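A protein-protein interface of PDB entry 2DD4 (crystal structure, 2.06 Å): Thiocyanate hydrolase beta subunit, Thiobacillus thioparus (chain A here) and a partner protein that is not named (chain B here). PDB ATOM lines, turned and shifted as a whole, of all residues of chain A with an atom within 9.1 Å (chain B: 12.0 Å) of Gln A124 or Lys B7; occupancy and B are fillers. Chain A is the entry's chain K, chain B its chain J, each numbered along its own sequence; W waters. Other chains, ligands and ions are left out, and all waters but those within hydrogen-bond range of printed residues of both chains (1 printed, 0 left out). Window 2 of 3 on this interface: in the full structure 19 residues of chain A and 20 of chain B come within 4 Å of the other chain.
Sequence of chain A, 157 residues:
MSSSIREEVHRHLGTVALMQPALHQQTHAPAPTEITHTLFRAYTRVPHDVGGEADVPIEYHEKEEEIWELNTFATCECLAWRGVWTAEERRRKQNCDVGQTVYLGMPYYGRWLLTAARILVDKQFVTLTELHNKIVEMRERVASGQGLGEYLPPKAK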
ATOM      1  N   VAL A  84       2.884 -23.912 -18.904  1.00  0.00           N
ATOM      2  CA  VAL A  84       3.969 -23.498 -18.021  1.00  0.00           C
ATOM      3  C   VAL A  84       4.567 -22.193 -18.554  1.00  0.00           C
ATOM      4  O   VAL A  84       5.036 -21.355 -17.787  1.00  0.00           O
ATOM      5  CB  VAL A  84       5.062 -24.584 -17.931  1.00  0.00           C
ATOM      6  CG1 VAL A  84       6.309 -24.029 -17.251  1.00  0.00           C
ATOM      7  CG2 VAL A  84       4.526 -25.772 -17.144  1.00  0.00           C
ATOM      8  N   ALA A 117      14.983 -26.329 -17.739  1.00  0.00           N
ATOM      9  CA  ALA A 117      15.244 -26.558 -16.323  1.00  0.00           C
ATOM     10  C   ALA A 117      15.009 -25.251 -15.580  1.00  0.00           C
ATOM     11  O   ALA A 117      14.480 -25.229 -14.465  1.00  0.00           O
ATOM     12  CB  ALA A 117      16.686 -27.009 -16.124  1.00  0.00           C
ATOM     13  N   ARG A 118      15.402 -24.157 -16.219  1.00  0.00           N
ATOM     14  CA  ARG A 118      15.266 -22.835 -15.635  1.00  0.00           C
ATOM     15  C   ARG A 118      13.813 -22.431 -15.379  1.00  0.00           C
ATOM     16  O   ARG A 118      13.487 -21.924 -14.303  1.00  0.00           O
ATOM     17  CB  ARG A 118      15.941 -21.806 -16.542  1.00  0.00           C
ATOM     18  CG  ARG A 118      16.056 -20.436 -15.929  1.00  0.00           C
ATOM     19  CD  ARG A 118      17.161 -20.353 -14.879  1.00  0.00           C
ATOM     20  NE  ARG A 118      16.919 -19.213 -14.002  1.00  0.00           N
ATOM     21  CZ  ARG A 118      17.857 -18.544 -13.341  1.00  0.00           C
ATOM     22  NH1 ARG A 118      19.133 -18.888 -13.447  1.00  0.00           N
ATOM     23  NH2 ARG A 118      17.508 -17.523 -12.570  1.00  0.00           N
ATOM     24  N   ILE A 119      12.933 -22.653 -16.353  1.00  0.00           N
ATOM     25  CA  ILE A 119      11.535 -22.274 -16.163  1.00  0.00           C
ATOM     26  C   ILE A 119      10.913 -23.016 -14.972  1.00  0.00           C
ATOM     27  O   ILE A 119      10.101 -22.447 -14.242  1.00  0.00           O
ATOM     28  CB  ILE A 119      10.690 -22.515 -17.448  1.00  0.00           C
ATOM     29  CG1 ILE A 119       9.352 -21.775 -17.334  1.00  0.00           C
ATOM     30  CG2 ILE A 119      10.448 -24.001 -17.656  1.00  0.00           C
ATOM     31  CD1 ILE A 119       9.485 -20.264 -17.141  1.00  0.00           C
ATOM     32  N   LEU A 120      11.299 -24.274 -14.762  1.00  0.00           N
ATOM     33  CA  LEU A 120      10.768 -25.042 -13.634  1.00  0.00           C
ATOM     34  C   LEU A 120      11.131 -24.375 -12.303  1.00  0.00           C
ATOM     35  O   LEU A 120      10.321 -24.331 -11.375  1.00  0.00           O
ATOM     36  CB  LEU A 120      11.325 -26.469 -13.628  1.00  0.00           C
ATOM     37  CG  LEU A 120      11.082 -27.367 -14.842  1.00  0.00           C
ATOM     38  CD1 LEU A 120      11.524 -28.785 -14.505  1.00  0.00           C
ATOM     39  CD2 LEU A 120       9.620 -27.351 -15.221  1.00  0.00           C
ATOM     40  N   VAL A 121      12.357 -23.864 -12.217  1.00  0.00           N
ATOM     41  CA  VAL A 121      12.835 -23.214 -11.002  1.00  0.00           C
ATOM     42  C   VAL A 121      12.321 -21.788 -10.824  1.00  0.00           C
ATOM     43  O   VAL A 121      11.877 -21.415  -9.737  1.00  0.00           O
ATOM     44  CB  VAL A 121      14.379 -23.183 -10.960  1.00  0.00           C
ATOM     45  CG1 VAL A 121      14.850 -22.418  -9.732  1.00  0.00           C
ATOM     46  CG2 VAL A 121      14.923 -24.608 -10.939  1.00  0.00           C
ATOM     47  N   ASP A 122      12.383 -20.993 -11.887  1.00  0.00           N
ATOM     48  CA  ASP A 122      11.939 -19.608 -11.819  1.00  0.00           C
ATOM     49  C   ASP A 122      10.454 -19.443 -11.503  1.00  0.00           C
ATOM     50  O   ASP A 122      10.066 -18.475 -10.851  1.00  0.00           O
ATOM     51  CB  ASP A 122      12.289 -18.869 -13.114  1.00  0.00           C
ATOM     52  CG  ASP A 122      13.780 -18.590 -13.237  1.00  0.00           C
ATOM     53  OD1 ASP A 122      14.418 -18.324 -12.198  1.00  0.00           O
ATOM     54  OD2 ASP A 122      14.311 -18.620 -14.368  1.00  0.00           O
ATOM     55  N   LYS A 123       9.619 -20.372 -11.960  1.00  0.00           N
ATOM     56  CA  LYS A 123       8.194 -20.278 -11.664  1.00  0.00           C
ATOM     57  C   LYS A 123       7.835 -21.145 -10.463  1.00  0.00           C
ATOM     58  O   LYS A 123       6.662 -21.402 -10.176  1.00  0.00           O
ATOM     59  CB  LYS A 123       7.353 -20.635 -12.896  1.00  0.00           C
ATOM     60  CG  LYS A 123       7.310 -19.478 -13.896  1.00  0.00           C
ATOM     61  CD  LYS A 123       6.353 -19.703 -15.058  1.00  0.00           C
ATOM     62  CE  LYS A 123       6.260 -18.439 -15.920  1.00  0.00           C
ATOM     63  NZ  LYS A 123       5.406 -18.603 -17.139  1.00  0.00           N
ATOM     64  N   GLN A 124       8.875 -21.587  -9.762  1.00  0.00           N
ATOM     65  CA  GLN A 124       8.737 -22.383  -8.551  1.00  0.00           C
ATOM     66  C   GLN A 124       7.913 -23.670  -8.638  1.00  0.00           C
ATOM     67  O   GLN A 124       7.213 -24.024  -7.691  1.00  0.00           O
ATOM     68  CB  GLN A 124       8.199 -21.487  -7.425  1.00  0.00           C
ATOM     69  CG  GLN A 124       9.195 -20.408  -6.992  1.00  0.00           C
ATOM     70  CD  GLN A 124       8.595 -19.371  -6.052  1.00  0.00           C
ATOM     71  OE1 GLN A 124       7.722 -18.598  -6.439  1.00  0.00           O
ATOM     72  NE2 GLN A 124       9.064 -19.356  -4.811  1.00  0.00           N
ATOM     73  N   PHE A 125       7.989 -24.371  -9.766  1.00  0.00           N
ATOM     74  CA  PHE A 125       7.273 -25.635  -9.892  1.00  0.00           C
ATOM     75  C   PHE A 125       8.130 -26.701  -9.222  1.00  0.00           C
ATOM     76  O   PHE A 125       7.642 -27.759  -8.824  1.00  0.00           O
ATOM     77  CB  PHE A 125       7.008 -25.960 -11.362  1.00  0.00           C
ATOM     78  CG  PHE A 125       5.982 -25.062 -11.988  1.00  0.00           C
ATOM     79  CD1 PHE A 125       4.692 -25.003 -11.467  1.00  0.00           C
ATOM     80  CD2 PHE A 125       6.306 -24.257 -13.074  1.00  0.00           C
ATOM     81  CE1 PHE A 125       3.735 -24.149 -12.021  1.00  0.00           C
ATOM     82  CE2 PHE A 125       5.357 -23.401 -13.635  1.00  0.00           C
ATOM     83  CZ  PHE A 125       4.071 -23.347 -13.107  1.00  0.00           C
ATOM     84  N   VAL A 126       9.419 -26.396  -9.099  1.00  0.00           N
ATOM     85  CA  VAL A 126      10.383 -27.257  -8.422  1.00  0.00           C
ATOM     86  C   VAL A 126      11.350 -26.289  -7.747  1.00  0.00           C
ATOM     87  O   VAL A 126      11.536 -25.167  -8.219  1.00  0.00           O
ATOM     88  CB  VAL A 126      11.209 -28.159  -9.392  1.00  0.00           C
ATOM     89  CG1 VAL A 126      10.286 -28.901 -10.349  1.00  0.00           C
ATOM     90  CG2 VAL A 126      12.236 -27.326 -10.141  1.00  0.00           C
ATOM     91  N   THR A 127      11.939 -26.699  -6.631  1.00  0.00           N
ATOM     92  CA  THR A 127      12.909 -25.845  -5.951  1.00  0.00           C
ATOM     93  C   THR A 127      14.244 -26.193  -6.595  1.00  0.00           C
ATOM     94  O   THR A 127      14.377 -27.266  -7.190  1.00  0.00           O
ATOM     95  CB  THR A 127      13.006 -26.165  -4.452  1.00  0.00           C
ATOM     96  OG1 THR A 127      13.458 -27.515  -4.292  1.00  0.00           O
ATOM     97  CG2 THR A 127      11.645 -25.994  -3.772  1.00  0.00           C
ATOM     98  N   LEU A 128      15.227 -25.302  -6.497  1.00  0.00           N
ATOM     99  CA  LEU A 128      16.530 -25.588  -7.080  1.00  0.00           C
ATOM    100  C   LEU A 128      17.096 -26.825  -6.389  1.00  0.00           C
ATOM    101  O   LEU A 128      17.829 -27.610  -6.996  1.00  0.00           O
ATOM    102  CB  LEU A 128      17.486 -24.401  -6.900  1.00  0.00           C
ATOM    103  CG  LEU A 128      18.869 -24.575  -7.552  1.00  0.00           C
ATOM    104  CD1 LEU A 128      18.704 -24.697  -9.061  1.00  0.00           C
ATOM    105  CD2 LEU A 128      19.769 -23.392  -7.216  1.00  0.00           C
ATOM    106  N   GLU A 130      15.435 -29.425  -5.401  1.00  0.00           N
ATOM    107  CA  GLU A 130      14.865 -30.605  -6.044  1.00  0.00           C
ATOM    108  C   GLU A 130      15.612 -30.883  -7.344  1.00  0.00           C
ATOM    109  O   GLU A 130      15.898 -32.034  -7.670  1.00  0.00           O
ATOM    110  CB  GLU A 130      13.376 -30.395  -6.335  1.00  0.00           C
ATOM    111  CG  GLU A 130      12.500 -30.436  -5.094  1.00  0.00           C
ATOM    112  CD  GLU A 130      11.039 -30.171  -5.403  1.00  0.00           C
ATOM    113  OE1 GLU A 130      10.745 -29.136  -6.037  1.00  0.00           O
ATOM    114  OE2 GLU A 130      10.187 -30.992  -5.007  1.00  0.00           O
ATOM    115  N   LYS B   7       3.049 -18.352  -1.850  1.00  0.00           N
ATOM    116  CA  LYS B   7       3.797 -18.180  -3.129  1.00  0.00           C
ATOM    117  C   LYS B   7       2.848 -17.858  -4.277  1.00  0.00           C
ATOM    118  O   LYS B   7       1.637 -18.054  -4.169  1.00  0.00           O
ATOM    119  CB  LYS B   7       4.584 -19.452  -3.461  1.00  0.00           C
ATOM    120  CG  LYS B   7       5.719 -19.762  -2.496  1.00  0.00           C
ATOM    121  CD  LYS B   7       6.459 -21.024  -2.918  1.00  0.00           C
ATOM    122  CE  LYS B   7       7.601 -21.351  -1.967  1.00  0.00           C
ATOM    123  NZ  LYS B   7       8.303 -22.611  -2.357  1.00  0.00           N
ATOM    124  N   PRO B   8       3.390 -17.349  -5.395  1.00  0.00           N
ATOM    125  CA  PRO B   8       2.572 -17.004  -6.561  1.00  0.00           C
ATOM    126  C   PRO B   8       1.977 -18.242  -7.223  1.00  0.00           C
ATOM    127  O   PRO B   8       2.551 -19.329  -7.162  1.00  0.00           O
ATOM    128  CB  PRO B   8       3.567 -16.301  -7.487  1.00  0.00           C
ATOM    129  CG  PRO B   8       4.598 -15.761  -6.548  1.00  0.00           C
ATOM    130  CD  PRO B   8       4.777 -16.895  -5.582  1.00  0.00           C
ATOM    131  N   VAL B   9       0.821 -18.071  -7.851  1.00  0.00           N
ATOM    132  CA  VAL B   9       0.164 -19.169  -8.546  1.00  0.00           C
ATOM    133  C   VAL B   9       0.091 -18.785 -10.014  1.00  0.00           C
ATOM    134  O   VAL B   9      -0.359 -17.690 -10.351  1.00  0.00           O
ATOM    135  CB  VAL B   9      -1.265 -19.404  -8.026  1.00  0.00           C
ATOM    136  CG1 VAL B   9      -1.904 -20.559  -8.785  1.00  0.00           C
ATOM    137  CG2 VAL B   9      -1.236 -19.694  -6.535  1.00  0.00           C
ATOM    138  N   TRP B  10       0.541 -19.680 -10.886  1.00  0.00           N
ATOM    139  CA  TRP B  10       0.521 -19.406 -12.314  1.00  0.00           C
ATOM    140  C   TRP B  10      -0.655 -20.089 -12.990  1.00  0.00           C
ATOM    141  O   TRP B  10      -0.904 -21.275 -12.781  1.00  0.00           O
ATOM    142  CB  TRP B  10       1.833 -19.857 -12.954  1.00  0.00           C
ATOM    143  CG  TRP B  10       3.026 -19.274 -12.274  1.00  0.00           C
ATOM    144  CD1 TRP B  10       3.644 -19.748 -11.150  1.00  0.00           C
ATOM    145  CD2 TRP B  10       3.704 -18.066 -12.626  1.00  0.00           C
ATOM    146  NE1 TRP B  10       4.665 -18.908 -10.779  1.00  0.00           N
ATOM    147  CE2 TRP B  10       4.724 -17.866 -11.668  1.00  0.00           C
ATOM    148  CE3 TRP B  10       3.551 -17.130 -13.657  1.00  0.00           C
ATOM    149  CZ2 TRP B  10       5.587 -16.768 -11.711  1.00  0.00           C
ATOM    150  CZ3 TRP B  10       4.411 -16.036 -13.700  1.00  0.00           C
ATOM    151  CH2 TRP B  10       5.416 -15.866 -12.731  1.00  0.00           C
ATOM    152  N   ASP B  11      -1.384 -19.325 -13.797  1.00  0.00           N
ATOM    153  CA  ASP B  11      -2.536 -19.850 -14.511  1.00  0.00           C
ATOM    154  C   ASP B  11      -2.039 -20.621 -15.727  1.00  0.00           C
ATOM    155  O   ASP B  11      -1.663 -20.027 -16.736  1.00  0.00           O
ATOM    156  CB  ASP B  11      -3.443 -18.708 -14.967  1.00  0.00           C
ATOM    157  CG  ASP B  11      -4.741 -19.204 -15.560  1.00  0.00           C
ATOM    158  OD1 ASP B  11      -4.735 -20.294 -16.167  1.00  0.00           O
ATOM    159  OD2 ASP B  11      -5.764 -18.503 -15.430  1.00  0.00           O
ATOM    160  N   ARG B  12      -2.043 -21.944 -15.632  1.00  0.00           N
ATOM    161  CA  ARG B  12      -1.567 -22.770 -16.728  1.00  0.00           C
ATOM    162  C   ARG B  12      -2.649 -23.181 -17.723  1.00  0.00           C
ATOM    163  O   ARG B  12      -2.371 -23.927 -18.662  1.00  0.00           O
ATOM    164  CB  ARG B  12      -0.876 -24.018 -16.174  1.00  0.00           C
ATOM    165  CG  ARG B  12       0.173 -23.707 -15.125  1.00  0.00           C
ATOM    166  CD  ARG B  12       1.330 -24.682 -15.185  1.00  0.00           C
ATOM    167  NE  ARG B  12       0.915 -26.070 -15.026  1.00  0.00           N
ATOM    168  CZ  ARG B  12       0.498 -26.611 -13.887  1.00  0.00           C
ATOM    169  NH1 ARG B  12       0.434 -25.881 -12.785  1.00  0.00           N
ATOM    170  NH2 ARG B  12       0.159 -27.893 -13.849  1.00  0.00           N
HETATM  171  O   HOH W   1       7.011 -17.931  -9.103  1.00  0.00           O
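The backbone carbonyl oxygen (O) of Lys A123 sits at hydrogen-bond distance from the indole nitrogen (NE1) of Trp B10 (3.3 Å).
O of Leu A120 lies within hydrogen-bond range of N of Phe A125, at 2.8 Å.
The backbone carbonyl oxygen (O) of Val A84 sits at hydrogen-bond distance from the side-chain amino group (NZ) of Lys A123 (2.9 Å).
Among the printed residues, pairs that only touch across the chains: Val A84 with Arg B12 (3.9 Å), Gln A124 with Lys B7 (3.6 Å), Gln A124 with Pro B8 (3.5 Å) and Phe A125 with Arg B12 (3.7 Å).
Gln A124 touches just these residues of chain B: Lys B7 and Pro B8.
Of chain A, only Gln A124 (3.6 Å) comes within 4 Å of Lys B7.
No residue of chain B comes within 4 Å of Val A121.
No residue of chain B comes within 4 Å of Asp A122.
Phe A125 touches just one residue of chain B: Arg B12 (3.7 Å).
Val A126 touches none of the printed residues of chain B.
Pro B8 touches just one residue of chain A: Gln A124.
Of the printed residues of chain A, Trp B10 touches Lys A123 (3.3 Å).
Printed residues of chain B within 4 Å of Lys A123: Trp B10 (3.3 Å).
Of the printed residues of chain A, Arg B12 touches Val A84 and Phe A125.
Of the printed residues of chain B, Val A84 touches Arg B12 (3.9 Å).
Leu A128 touches none of the printed residues of chain B.
The nearest printed residue of chain A that does not touch Trp B10 is Phe A125 (4.1 Å).
Hydrophobic or aromatic side chains of chain B that line the printed part of chain A: Pro B8 and Trp B10.
Of the 14 printed residues of chain A, 4 touch a printed residue of chain B.
Printed residues of chain A that touch a printed residue of chain B: Val A84, Lys A123, Gln A124 and Phe A125.
Hydrophobic or aromatic side chains of chain A within 4 Å of the printed part of chain B: Val A84 and Phe A125.
Along chain A the printed residues that touch a printed residue of chain B span positions 84 to 125.
Among the printed residues, 5 pairs touch across the chains.
Water W1 bridges the side-chain amide oxygen of Gln A124 (2.8 Å) and the indole nitrogen of Trp B10 (3.0 Å).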
